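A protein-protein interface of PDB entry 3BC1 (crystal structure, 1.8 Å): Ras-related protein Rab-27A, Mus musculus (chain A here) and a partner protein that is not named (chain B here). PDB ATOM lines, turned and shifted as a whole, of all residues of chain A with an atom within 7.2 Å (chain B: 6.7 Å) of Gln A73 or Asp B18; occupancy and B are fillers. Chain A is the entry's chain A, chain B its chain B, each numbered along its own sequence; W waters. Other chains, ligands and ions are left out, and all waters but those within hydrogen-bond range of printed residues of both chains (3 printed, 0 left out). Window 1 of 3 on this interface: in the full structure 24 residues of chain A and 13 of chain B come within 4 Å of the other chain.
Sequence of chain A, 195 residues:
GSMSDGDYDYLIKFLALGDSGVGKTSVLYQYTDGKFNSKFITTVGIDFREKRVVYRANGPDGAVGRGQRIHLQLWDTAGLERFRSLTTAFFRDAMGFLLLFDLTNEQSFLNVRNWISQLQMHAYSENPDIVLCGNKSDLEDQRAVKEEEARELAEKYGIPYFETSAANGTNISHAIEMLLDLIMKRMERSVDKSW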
ATOM      1  N   LEU A  11      -5.390 -15.339  27.130  1.00  0.00           N
ATOM      2  CA  LEU A  11      -6.591 -14.564  26.831  1.00  0.00           C
ATOM      3  C   LEU A  11      -7.754 -15.545  26.799  1.00  0.00           C
ATOM      4  O   LEU A  11      -7.784 -16.456  25.961  1.00  0.00           O
ATOM      5  CB  LEU A  11      -6.482 -13.822  25.488  1.00  0.00           C
ATOM      6  CG  LEU A  11      -7.734 -13.058  25.016  1.00  0.00           C
ATOM      7  CD1 LEU A  11      -8.145 -12.011  26.025  1.00  0.00           C
ATOM      8  CD2 LEU A  11      -7.527 -12.412  23.650  1.00  0.00           C
ATOM      9  N   ILE A  12      -8.695 -15.360  27.723  1.00  0.00           N
ATOM     10  CA  ILE A  12      -9.877 -16.206  27.824  1.00  0.00           C
ATOM     11  C   ILE A  12     -11.098 -15.367  27.464  1.00  0.00           C
ATOM     12  O   ILE A  12     -11.266 -14.267  27.977  1.00  0.00           O
ATOM     13  CB  ILE A  12     -10.040 -16.782  29.237  1.00  0.00           C
ATOM     14  CG1 ILE A  12      -8.805 -17.604  29.633  1.00  0.00           C
ATOM     15  CG2 ILE A  12     -11.283 -17.643  29.317  1.00  0.00           C
ATOM     16  CD1 ILE A  12      -8.610 -18.857  28.809  1.00  0.00           C
ATOM     17  N   LYS A  13     -11.926 -15.882  26.558  1.00  0.00           N
ATOM     18  CA  LYS A  13     -13.089 -15.148  26.054  1.00  0.00           C
ATOM     19  C   LYS A  13     -14.381 -15.828  26.498  1.00  0.00           C
ATOM     20  O   LYS A  13     -14.591 -17.012  26.221  1.00  0.00           O
ATOM     21  CB  LYS A  13     -13.043 -15.044  24.520  1.00  0.00           C
ATOM     22  CG  LYS A  13     -11.748 -14.444  23.966  1.00  0.00           C
ATOM     23  CD  LYS A  13     -11.759 -14.340  22.443  1.00  0.00           C
ATOM     24  CE  LYS A  13     -10.406 -13.860  21.916  1.00  0.00           C
ATOM     25  NZ  LYS A  13     -10.377 -13.604  20.434  1.00  0.00           N
ATOM     26  N   PHE A  14     -15.233 -15.084  27.204  1.00  0.00           N
ATOM     27  CA  PHE A  14     -16.558 -15.567  27.591  1.00  0.00           C
ATOM     28  C   PHE A  14     -17.647 -14.699  26.975  1.00  0.00           C
ATOM     29  O   PHE A  14     -17.393 -13.570  26.561  1.00  0.00           O
ATOM     30  CB  PHE A  14     -16.740 -15.570  29.116  1.00  0.00           C
ATOM     31  CG  PHE A  14     -15.860 -16.558  29.846  1.00  0.00           C
ATOM     32  CD1 PHE A  14     -15.534 -17.785  29.281  1.00  0.00           C
ATOM     33  CD2 PHE A  14     -15.396 -16.270  31.119  1.00  0.00           C
ATOM     34  CE1 PHE A  14     -14.731 -18.692  29.962  1.00  0.00           C
ATOM     35  CE2 PHE A  14     -14.596 -17.179  31.809  1.00  0.00           C
ATOM     36  CZ  PHE A  14     -14.271 -18.390  31.221  1.00  0.00           C
ATOM     37  N   LEU A  15     -18.861 -15.236  26.924  1.00  0.00           N
ATOM     38  CA  LEU A  15     -20.010 -14.483  26.422  1.00  0.00           C
ATOM     39  C   LEU A  15     -21.236 -14.618  27.325  1.00  0.00           C
ATOM     40  O   LEU A  15     -21.627 -15.726  27.710  1.00  0.00           O
ATOM     41  CB  LEU A  15     -20.354 -14.926  24.999  1.00  0.00           C
ATOM     42  CG  LEU A  15     -21.451 -14.145  24.261  1.00  0.00           C
ATOM     43  CD1 LEU A  15     -21.161 -14.046  22.757  1.00  0.00           C
ATOM     44  CD2 LEU A  15     -22.817 -14.773  24.491  1.00  0.00           C
ATOM     45  N   PHE A  48     -18.341  -5.489  24.830  1.00  0.00           N
ATOM     46  CA  PHE A  48     -17.540  -6.337  25.714  1.00  0.00           C
ATOM     47  C   PHE A  48     -16.835  -5.536  26.791  1.00  0.00           C
ATOM     48  O   PHE A  48     -16.634  -4.330  26.666  1.00  0.00           O
ATOM     49  CB  PHE A  48     -16.531  -7.192  24.924  1.00  0.00           C
ATOM     50  CG  PHE A  48     -15.387  -6.420  24.339  1.00  0.00           C
ATOM     51  CD1 PHE A  48     -14.221  -6.218  25.072  1.00  0.00           C
ATOM     52  CD2 PHE A  48     -15.459  -5.916  23.049  1.00  0.00           C
ATOM     53  CE1 PHE A  48     -13.150  -5.516  24.539  1.00  0.00           C
ATOM     54  CE2 PHE A  48     -14.391  -5.213  22.503  1.00  0.00           C
ATOM     55  CZ  PHE A  48     -13.237  -5.005  23.248  1.00  0.00           C
ATOM     56  N   ARG A  49     -16.466  -6.235  27.857  1.00  0.00           N
ATOM     57  CA  ARG A  49     -15.678  -5.667  28.937  1.00  0.00           C
ATOM     58  C   ARG A  49     -14.464  -6.554  29.161  1.00  0.00           C
ATOM     59  O   ARG A  49     -14.392  -7.673  28.635  1.00  0.00           O
ATOM     60  CB  ARG A  49     -16.523  -5.578  30.211  1.00  0.00           C
ATOM     61  CG  ARG A  49     -17.815  -4.772  30.044  1.00  0.00           C
ATOM     62  CD  ARG A  49     -18.303  -4.214  31.372  1.00  0.00           C
ATOM     63  NE  ARG A  49     -17.367  -3.217  31.887  1.00  0.00           N
ATOM     64  CZ  ARG A  49     -17.380  -1.922  31.571  1.00  0.00           C
ATOM     65  NH1 ARG A  49     -18.288  -1.421  30.733  1.00  0.00           N
ATOM     66  NH2 ARG A  49     -16.462  -1.117  32.097  1.00  0.00           N
ATOM     67  N   GLU A  50     -13.504  -6.045  29.921  1.00  0.00           N
ATOM     68  CA  GLU A  50     -12.266  -6.771  30.176  1.00  0.00           C
ATOM     69  C   GLU A  50     -11.882  -6.741  31.647  1.00  0.00           C
ATOM     70  O   GLU A  50     -12.218  -5.804  32.377  1.00  0.00           O
ATOM     71  CB  GLU A  50     -11.109  -6.175  29.372  1.00  0.00           C
ATOM     72  CG  GLU A  50     -11.332  -6.062  27.873  1.00  0.00           C
ATOM     73  CD  GLU A  50     -10.288  -5.181  27.233  1.00  0.00           C
ATOM     74  OE1 GLU A  50      -9.129  -5.620  27.111  1.00  0.00           O
ATOM     75  OE2 GLU A  50     -10.616  -4.033  26.884  1.00  0.00           O
ATOM     76  N   LYS A  51     -11.150  -7.765  32.070  1.00  0.00           N
ATOM     77  CA  LYS A  51     -10.613  -7.803  33.422  1.00  0.00           C
ATOM     78  C   LYS A  51      -9.390  -8.689  33.478  1.00  0.00           C
ATOM     79  O   LYS A  51      -9.363  -9.759  32.873  1.00  0.00           O
ATOM     80  CB  LYS A  51     -11.661  -8.291  34.427  1.00  0.00           C
ATOM     81  CG  LYS A  51     -11.243  -8.031  35.867  1.00  0.00           C
ATOM     82  CD  LYS A  51     -12.285  -8.431  36.882  1.00  0.00           C
ATOM     83  CE  LYS A  51     -11.929  -7.845  38.255  1.00  0.00           C
ATOM     84  NZ  LYS A  51     -12.964  -8.096  39.278  1.00  0.00           N
ATOM     85  N   ILE A  70      -4.552 -14.178  33.683  1.00  0.00           N
ATOM     86  CA  ILE A  70      -5.602 -14.271  32.680  1.00  0.00           C
ATOM     87  C   ILE A  70      -6.091 -12.877  32.315  1.00  0.00           C
ATOM     88  O   ILE A  70      -6.408 -12.077  33.189  1.00  0.00           O
ATOM     89  CB  ILE A  70      -6.830 -15.077  33.178  1.00  0.00           C
ATOM     90  CG1 ILE A  70      -6.423 -16.431  33.772  1.00  0.00           C
ATOM     91  CG2 ILE A  70      -7.831 -15.274  32.043  1.00  0.00           C
ATOM     92  CD1 ILE A  70      -5.672 -17.324  32.830  1.00  0.00           C
ATOM     93  N   HIS A  71      -6.151 -12.596  31.019  1.00  0.00           N
ATOM     94  CA  HIS A  71      -6.913 -11.454  30.527  1.00  0.00           C
ATOM     95  C   HIS A  71      -8.280 -11.958  30.079  1.00  0.00           C
ATOM     96  O   HIS A  71      -8.381 -12.736  29.126  1.00  0.00           O
ATOM     97  CB  HIS A  71      -6.203 -10.762  29.370  1.00  0.00           C
ATOM     98  CG  HIS A  71      -6.778  -9.420  29.050  1.00  0.00           C
ATOM     99  ND1 HIS A  71      -6.538  -8.308  29.828  1.00  0.00           N
ATOM    100  CD2 HIS A  71      -7.610  -9.017  28.061  1.00  0.00           C
ATOM    101  CE1 HIS A  71      -7.183  -7.272  29.321  1.00  0.00           C
ATOM    102  NE2 HIS A  71      -7.841  -7.676  28.249  1.00  0.00           N
ATOM    103  N   LEU A  72      -9.323 -11.534  30.783  1.00  0.00           N
ATOM    104  CA  LEU A  72     -10.688 -11.918  30.448  1.00  0.00           C
ATOM    105  C   LEU A  72     -11.272 -10.913  29.464  1.00  0.00           C
ATOM    106  O   LEU A  72     -11.210  -9.711  29.705  1.00  0.00           O
ATOM    107  CB  LEU A  72     -11.574 -11.977  31.699  1.00  0.00           C
ATOM    108  CG  LEU A  72     -11.368 -13.111  32.699  1.00  0.00           C
ATOM    109  CD1 LEU A  72     -12.116 -12.822  33.997  1.00  0.00           C
ATOM    110  CD2 LEU A  72     -11.831 -14.438  32.087  1.00  0.00           C
ATOM    111  N   GLN A  73     -11.805 -11.406  28.349  1.00  0.00           N
ATOM    112  CA  GLN A  73     -12.678 -10.608  27.493  1.00  0.00           C
ATOM    113  C   GLN A  73     -14.090 -11.150  27.663  1.00  0.00           C
ATOM    114  O   GLN A  73     -14.362 -12.313  27.355  1.00  0.00           O
ATOM    115  CB  GLN A  73     -12.245 -10.667  26.023  1.00  0.00           C
ATOM    116  CG  GLN A  73     -13.114  -9.818  25.093  1.00  0.00           C
ATOM    117  CD  GLN A  73     -12.734  -9.926  23.622  1.00  0.00           C
ATOM    118  OE1 GLN A  73     -12.264 -10.961  23.158  1.00  0.00           O
ATOM    119  NE2 GLN A  73     -12.953  -8.852  22.882  1.00  0.00           N
ATOM    120  N   LEU A  74     -14.987 -10.307  28.160  1.00  0.00           N
ATOM    121  CA  LEU A  74     -16.326 -10.730  28.525  1.00  0.00           C
ATOM    122  C   LEU A  74     -17.312 -10.090  27.559  1.00  0.00           C
ATOM    123  O   LEU A  74     -17.630  -8.906  27.680  1.00  0.00           O
ATOM    124  CB  LEU A  74     -16.625 -10.336  29.978  1.00  0.00           C
ATOM    125  CG  LEU A  74     -15.537 -10.780  30.977  1.00  0.00           C
ATOM    126  CD1 LEU A  74     -15.705 -10.109  32.329  1.00  0.00           C
ATOM    127  CD2 LEU A  74     -15.525 -12.290  31.116  1.00  0.00           C
ATOM    128  N   TRP A  75     -17.760 -10.870  26.580  1.00  0.00           N
ATOM    129  CA  TRP A  75     -18.687 -10.370  25.565  1.00  0.00           C
ATOM    130  C   TRP A  75     -20.076 -10.202  26.134  1.00  0.00           C
ATOM    131  O   TRP A  75     -20.571 -11.054  26.879  1.00  0.00           O
ATOM    132  CB  TRP A  75     -18.743 -11.296  24.350  1.00  0.00           C
ATOM    133  CG  TRP A  75     -17.558 -11.155  23.490  1.00  0.00           C
ATOM    134  CD1 TRP A  75     -16.424 -11.907  23.535  1.00  0.00           C
ATOM    135  CD2 TRP A  75     -17.358 -10.181  22.460  1.00  0.00           C
ATOM    136  NE1 TRP A  75     -15.527 -11.469  22.585  1.00  0.00           N
ATOM    137  CE2 TRP A  75     -16.078 -10.412  21.912  1.00  0.00           C
ATOM    138  CE3 TRP A  75     -18.137  -9.141  21.942  1.00  0.00           C
ATOM    139  CZ2 TRP A  75     -15.557  -9.639  20.871  1.00  0.00           C
ATOM    140  CZ3 TRP A  75     -17.622  -8.377  20.910  1.00  0.00           C
ATOM    141  CH2 TRP A  75     -16.343  -8.633  20.383  1.00  0.00           C
ATOM    142  N   ASP A  76     -20.690  -9.089  25.759  1.00  0.00           N
ATOM    143  CA  ASP A  76     -21.971  -8.683  26.271  1.00  0.00           C
ATOM    144  C   ASP A  76     -22.939  -8.553  25.101  1.00  0.00           C
ATOM    145  O   ASP A  76     -22.860  -7.584  24.333  1.00  0.00           O
ATOM    146  CB  ASP A  76     -21.800  -7.342  26.994  1.00  0.00           C
ATOM    147  CG  ASP A  76     -23.066  -6.865  27.654  1.00  0.00           C
ATOM    148  OD1 ASP A  76     -24.007  -7.675  27.791  1.00  0.00           O
ATOM    149  OD2 ASP A  76     -23.112  -5.667  28.032  1.00  0.00           O
ATOM    150  N   PHE A  90     -21.612 -14.354  17.190  1.00  0.00           N
ATOM    151  CA  PHE A  90     -20.523 -14.282  18.166  1.00  0.00           C
ATOM    152  C   PHE A  90     -20.457 -15.474  19.131  1.00  0.00           C
ATOM    153  O   PHE A  90     -19.486 -15.594  19.888  1.00  0.00           O
ATOM    154  CB  PHE A  90     -20.591 -12.949  18.930  1.00  0.00           C
ATOM    155  CG  PHE A  90     -19.949 -11.815  18.191  1.00  0.00           C
ATOM    156  CD1 PHE A  90     -20.656 -11.096  17.244  1.00  0.00           C
ATOM    157  CD2 PHE A  90     -18.617 -11.493  18.414  1.00  0.00           C
ATOM    158  CE1 PHE A  90     -20.059 -10.063  16.539  1.00  0.00           C
ATOM    159  CE2 PHE A  90     -18.013 -10.459  17.714  1.00  0.00           C
ATOM    160  CZ  PHE A  90     -18.738  -9.748  16.772  1.00  0.00           C
ATOM    161  N   ASP A  93     -17.178 -18.074  18.701  1.00  0.00           N
ATOM    162  CA  ASP A  93     -15.827 -17.719  19.149  1.00  0.00           C
ATOM    163  C   ASP A  93     -15.663 -17.642  20.680  1.00  0.00           C
ATOM    164  O   ASP A  93     -14.556 -17.404  21.167  1.00  0.00           O
ATOM    165  CB  ASP A  93     -15.328 -16.433  18.465  1.00  0.00           C
ATOM    166  CG  ASP A  93     -15.734 -15.160  19.195  1.00  0.00           C
ATOM    167  OD1 ASP A  93     -16.944 -14.970  19.469  1.00  0.00           O
ATOM    168  OD2 ASP A  93     -14.835 -14.323  19.461  1.00  0.00           O
ATOM    169  N   LYS B  13     -17.611   0.665  16.544  1.00  0.00           N
ATOM    170  CA  LYS B  13     -16.662   1.075  17.585  1.00  0.00           C
ATOM    171  C   LYS B  13     -16.266  -0.105  18.482  1.00  0.00           C
ATOM    172  O   LYS B  13     -15.105  -0.215  18.882  1.00  0.00           O
ATOM    173  CB  LYS B  13     -17.235   2.231  18.416  1.00  0.00           C
ATOM    174  CG  LYS B  13     -17.381   3.530  17.612  1.00  0.00           C
ATOM    175  CD  LYS B  13     -18.039   4.650  18.401  1.00  0.00           C
ATOM    176  CE  LYS B  13     -18.093   5.943  17.576  1.00  0.00           C
ATOM    177  NZ  LYS B  13     -18.639   7.093  18.354  1.00  0.00           N
ATOM    178  N   VAL B  14     -17.224  -0.976  18.789  1.00  0.00           N
ATOM    179  CA  VAL B  14     -16.945  -2.204  19.555  1.00  0.00           C
ATOM    180  C   VAL B  14     -16.016  -3.119  18.747  1.00  0.00           C
ATOM    181  O   VAL B  14     -15.014  -3.625  19.262  1.00  0.00           O
ATOM    182  CB  VAL B  14     -18.255  -2.947  19.942  1.00  0.00           C
ATOM    183  CG1 VAL B  14     -17.964  -4.313  20.590  1.00  0.00           C
ATOM    184  CG2 VAL B  14     -19.082  -2.087  20.888  1.00  0.00           C
ATOM    185  N   LEU B  15     -16.341  -3.310  17.474  1.00  0.00           N
ATOM    186  CA  LEU B  15     -15.530  -4.166  16.620  1.00  0.00           C
ATOM    187  C   LEU B  15     -14.108  -3.605  16.473  1.00  0.00           C
ATOM    188  O   LEU B  15     -13.155  -4.365  16.387  1.00  0.00           O
ATOM    189  CB  LEU B  15     -16.186  -4.347  15.253  1.00  0.00           C
ATOM    190  CG  LEU B  15     -17.518  -5.105  15.242  1.00  0.00           C
ATOM    191  CD1 LEU B  15     -18.040  -5.193  13.824  1.00  0.00           C
ATOM    192  CD2 LEU B  15     -17.377  -6.497  15.854  1.00  0.00           C
ATOM    193  N   GLN B  16     -13.975  -2.281  16.462  1.00  0.00           N
ATOM    194  CA  GLN B  16     -12.657  -1.653  16.365  1.00  0.00           C
ATOM    195  C   GLN B  16     -11.839  -1.905  17.627  1.00  0.00           C
ATOM    196  O   GLN B  16     -10.651  -2.203  17.544  1.00  0.00           O
ATOM    197  CB  GLN B  16     -12.787  -0.160  16.070  1.00  0.00           C
ATOM    198  CG  GLN B  16     -13.157   0.099  14.616  1.00  0.00           C
ATOM    199  CD  GLN B  16     -13.946   1.372  14.371  1.00  0.00           C
ATOM    200  OE1 GLN B  16     -14.070   2.239  15.245  1.00  0.00           O
ATOM    201  NE2 GLN B  16     -14.484   1.492  13.162  1.00  0.00           N
ATOM    202  N   ARG B  17     -12.485  -1.809  18.785  1.00  0.00           N
ATOM    203  CA  ARG B  17     -11.830  -2.109  20.056  1.00  0.00           C
ATOM    204  C   ARG B  17     -11.392  -3.570  20.146  1.00  0.00           C
ATOM    205  O   ARG B  17     -10.313  -3.866  20.658  1.00  0.00           O
ATOM    206  CB  ARG B  17     -12.761  -1.785  21.222  1.00  0.00           C
ATOM    207  CG  ARG B  17     -12.984  -0.291  21.456  1.00  0.00           C
ATOM    208  CD  ARG B  17     -14.205  -0.045  22.328  1.00  0.00           C
ATOM    209  NE  ARG B  17     -14.220  -0.925  23.492  1.00  0.00           N
ATOM    210  CZ  ARG B  17     -15.301  -1.511  24.005  1.00  0.00           C
ATOM    211  NH1 ARG B  17     -16.507  -1.335  23.476  1.00  0.00           N
ATOM    212  NH2 ARG B  17     -15.170  -2.299  25.058  1.00  0.00           N
ATOM    213  N   ASP B  18     -12.246  -4.471  19.668  1.00  0.00           N
ATOM    214  CA  ASP B  18     -11.922  -5.896  19.617  1.00  0.00           C
ATOM    215  C   ASP B  18     -10.714  -6.138  18.708  1.00  0.00           C
ATOM    216  O   ASP B  18      -9.838  -6.936  19.031  1.00  0.00           O
ATOM    217  CB  ASP B  18     -13.126  -6.708  19.130  1.00  0.00           C
ATOM    218  CG  ASP B  18     -12.850  -8.203  19.087  1.00  0.00           C
ATOM    219  OD1 ASP B  18     -12.361  -8.755  20.102  1.00  0.00           O
ATOM    220  OD2 ASP B  18     -13.140  -8.827  18.042  1.00  0.00           O
ATOM    221  N   ALA B  19     -10.675  -5.437  17.578  1.00  0.00           N
ATOM    222  CA  ALA B  19      -9.567  -5.564  16.632  1.00  0.00           C
ATOM    223  C   ALA B  19      -8.244  -5.152  17.268  1.00  0.00           C
ATOM    224  O   ALA B  19      -7.226  -5.816  17.081  1.00  0.00           O
ATOM    225  CB  ALA B  19      -9.833  -4.733  15.386  1.00  0.00           C
ATOM    226  N   ALA B  20      -8.267  -4.059  18.024  1.00  0.00           N
ATOM    227  CA  ALA B  20      -7.076  -3.585  18.728  1.00  0.00           C
ATOM    228  C   ALA B  20      -6.609  -4.597  19.781  1.00  0.00           C
ATOM    229  O   ALA B  20      -5.411  -4.854  19.898  1.00  0.00           O
ATOM    230  CB  ALA B  20      -7.330  -2.230  19.362  1.00  0.00           C
ATOM    231  N   LEU B  21      -7.549  -5.183  20.525  1.00  0.00           N
ATOM    232  CA  LEU B  21      -7.207  -6.220  21.511  1.00  0.00           C
ATOM    233  C   LEU B  21      -6.607  -7.452  20.834  1.00  0.00           C
ATOM    234  O   LEU B  21      -5.627  -8.019  21.317  1.00  0.00           O
ATOM    235  CB  LEU B  21      -8.432  -6.618  22.343  1.00  0.00           C
ATOM    236  CG  LEU B  21      -8.234  -7.759  23.356  1.00  0.00           C
ATOM    237  CD1 LEU B  21      -7.118  -7.443  24.349  1.00  0.00           C
ATOM    238  CD2 LEU B  21      -9.527  -8.058  24.110  1.00  0.00           C
ATOM    239  N   LYS B  22      -7.212  -7.864  19.724  1.00  0.00           N
ATOM    240  CA  LYS B  22      -6.707  -8.988  18.931  1.00  0.00           C
ATOM    241  C   LYS B  22      -5.286  -8.758  18.412  1.00  0.00           C
ATOM    242  O   LYS B  22      -4.459  -9.664  18.474  1.00  0.00           O
ATOM    243  CB  LYS B  22      -7.671  -9.313  17.782  1.00  0.00           C
ATOM    244  CG  LYS B  22      -8.827 -10.224  18.212  1.00  0.00           C
ATOM    245  CD  LYS B  22     -10.106 -10.047  17.381  1.00  0.00           C
ATOM    246  CE  LYS B  22      -9.875 -10.090  15.888  1.00  0.00           C
ATOM    247  NZ  LYS B  22     -11.155  -9.842  15.129  1.00  0.00           N
ATOM    248  N   ARG B  23      -4.996  -7.558  17.918  1.00  0.00           N
ATOM    249  CA  ARG B  23      -3.637  -7.237  17.456  1.00  0.00           C
ATOM    250  C   ARG B  23      -2.614  -7.280  18.604  1.00  0.00           C
ATOM    251  O   ARG B  23      -1.508  -7.819  18.443  1.00  0.00           O
ATOM    252  CB  ARG B  23      -3.605  -5.870  16.772  1.00  0.00           C
ATOM    253  CG  ARG B  23      -4.308  -5.836  15.413  1.00  0.00           C
ATOM    254  CD  ARG B  23      -3.525  -6.568  14.342  1.00  0.00           C
ATOM    255  NE  ARG B  23      -4.213  -6.540  13.049  1.00  0.00           N
ATOM    256  CZ  ARG B  23      -4.830  -7.571  12.468  1.00  0.00           C
ATOM    257  NH1 ARG B  23      -4.869  -8.773  13.030  1.00  0.00           N
ATOM    258  NH2 ARG B  23      -5.408  -7.389  11.287  1.00  0.00           N
HETATM  259  O   HOH W   1     -11.768 -11.269  20.514  1.00  0.00           O
HETATM  260  O   HOH W   2     -12.634  -2.582  27.073  1.00  0.00           O
HETATM  261  O   HOH W   3     -17.703  -1.477  27.323  1.00  0.00           O
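The guanidinium group (NH2) of Arg B17 lies within hydrogen-bond range of the backbone carbonyl oxygen (O) of Phe A48, at 3.0 Å.
The side-chain amide nitrogen (NE2) of Gln A73 sits at hydrogen-bond distance from the side-chain carboxylate (OD1) of Asp B18, at 2.8 Å.
The backbone NH of Gln A73 sits at hydrogen-bond distance from the backbone carbonyl oxygen of Ile A12, at 2.9 Å.
N of Phe A14 is in hydrogen-bond range of O of Gln A73 (2.9 Å).
The side-chain carboxylate (OE1) of Glu A50 sits at hydrogen-bond distance from a ring nitrogen (NE2) of His A71.
The side-chain amide oxygen (OE1) of Gln A73 sits at hydrogen-bond distance from the indole nitrogen (NE1) of Trp A75 (3.4 Å).
The side-chain carboxylate of Asp A93 sits close to the backbone carbonyl oxygen of Phe A90, at 2.7 Å.
OD2 of Asp B18 is in salt-bridge range of NZ of Lys B22 (3.7 Å).
O of Val B14 touches CE2 of Phe A48 (3.7 Å).
Asp B18 touches Phe A48.
OE1 of Glu A50 touches CD1 of Leu B21, at 3.9 Å.
Leu B21 touches His A71 (CD1 to NE2, 3.97 Å).
Leu B21 touches Gln A73.
Asp B18 touches Trp A75 (OD1 to CZ2, 3.4 Å).
Leu B15 touches Phe A90 (CD2 to CZ, 3.6 Å).
Gln A73 touches just these residues of chain B: Asp B18 and Leu B21.
Asp B18 touches three residues of chain A.
Printed residues of chain B within 4 Å of Phe A90: Leu B15 (3.6 Å).
Printed residues of chain A within 4 Å of Arg B17: Phe A48.
Of the printed residues of chain A, Leu B15 touches Phe A90.
Of the printed residues of chain A, Val B14 touches Phe A48 (3.7 Å).
Printed residues of chain A within 4 Å of Leu B21: Glu A50 (3.9 Å), His A71 (3.97 Å) and Gln A73 (3.7 Å).
Lys A13 touches none of the printed residues of chain B.
The nearest residue of chain A that does not touch Asp B18 is Phe A90 (5.1 Å).
The nearest printed residue of chain B that does not touch Trp A75 is Val B14 (4.1 Å).
Of the 18 printed residues of chain A, 6 touch a printed residue of chain B.
Printed residues of chain A that touch a printed residue of chain B: Phe A48, Glu A50, His A71, Gln A73, Trp A75 and Phe A90.
Of the 11 printed residues of chain B, 5 touch a printed residue of chain A.
Hydrophobic or aromatic side chains of chain B that line the printed part of chain A: Val B14, Leu B15 and Leu B21.
Along chain B the printed residues that touch a printed residue of chain A span positions 14 to 21.
Among the printed residues, no Asp or Glu carboxylate lies within 4 Å of a Lys or Arg side-chain nitrogen of the other chain.
Water W2 bridges OE2 of Glu A50 (2.5 Å) and NH2 of Arg B17 (3.3 Å).
Water W1 lies within hydrogen-bond range of the side-chain carboxylate (OD1) of Asp B18 (2.6 Å), the side-chain amide oxygen (OE1) of Gln A73 (2.7 Å) and the side-chain amino group (NZ) of Lys A13 (2.7 Å).
Water W3 lies within hydrogen-bond range of the backbone carbonyl oxygen (O) of Phe A48, the guanidinium group (NH1) of Arg A49 and the guanidinium group (NH2) of Arg B17.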
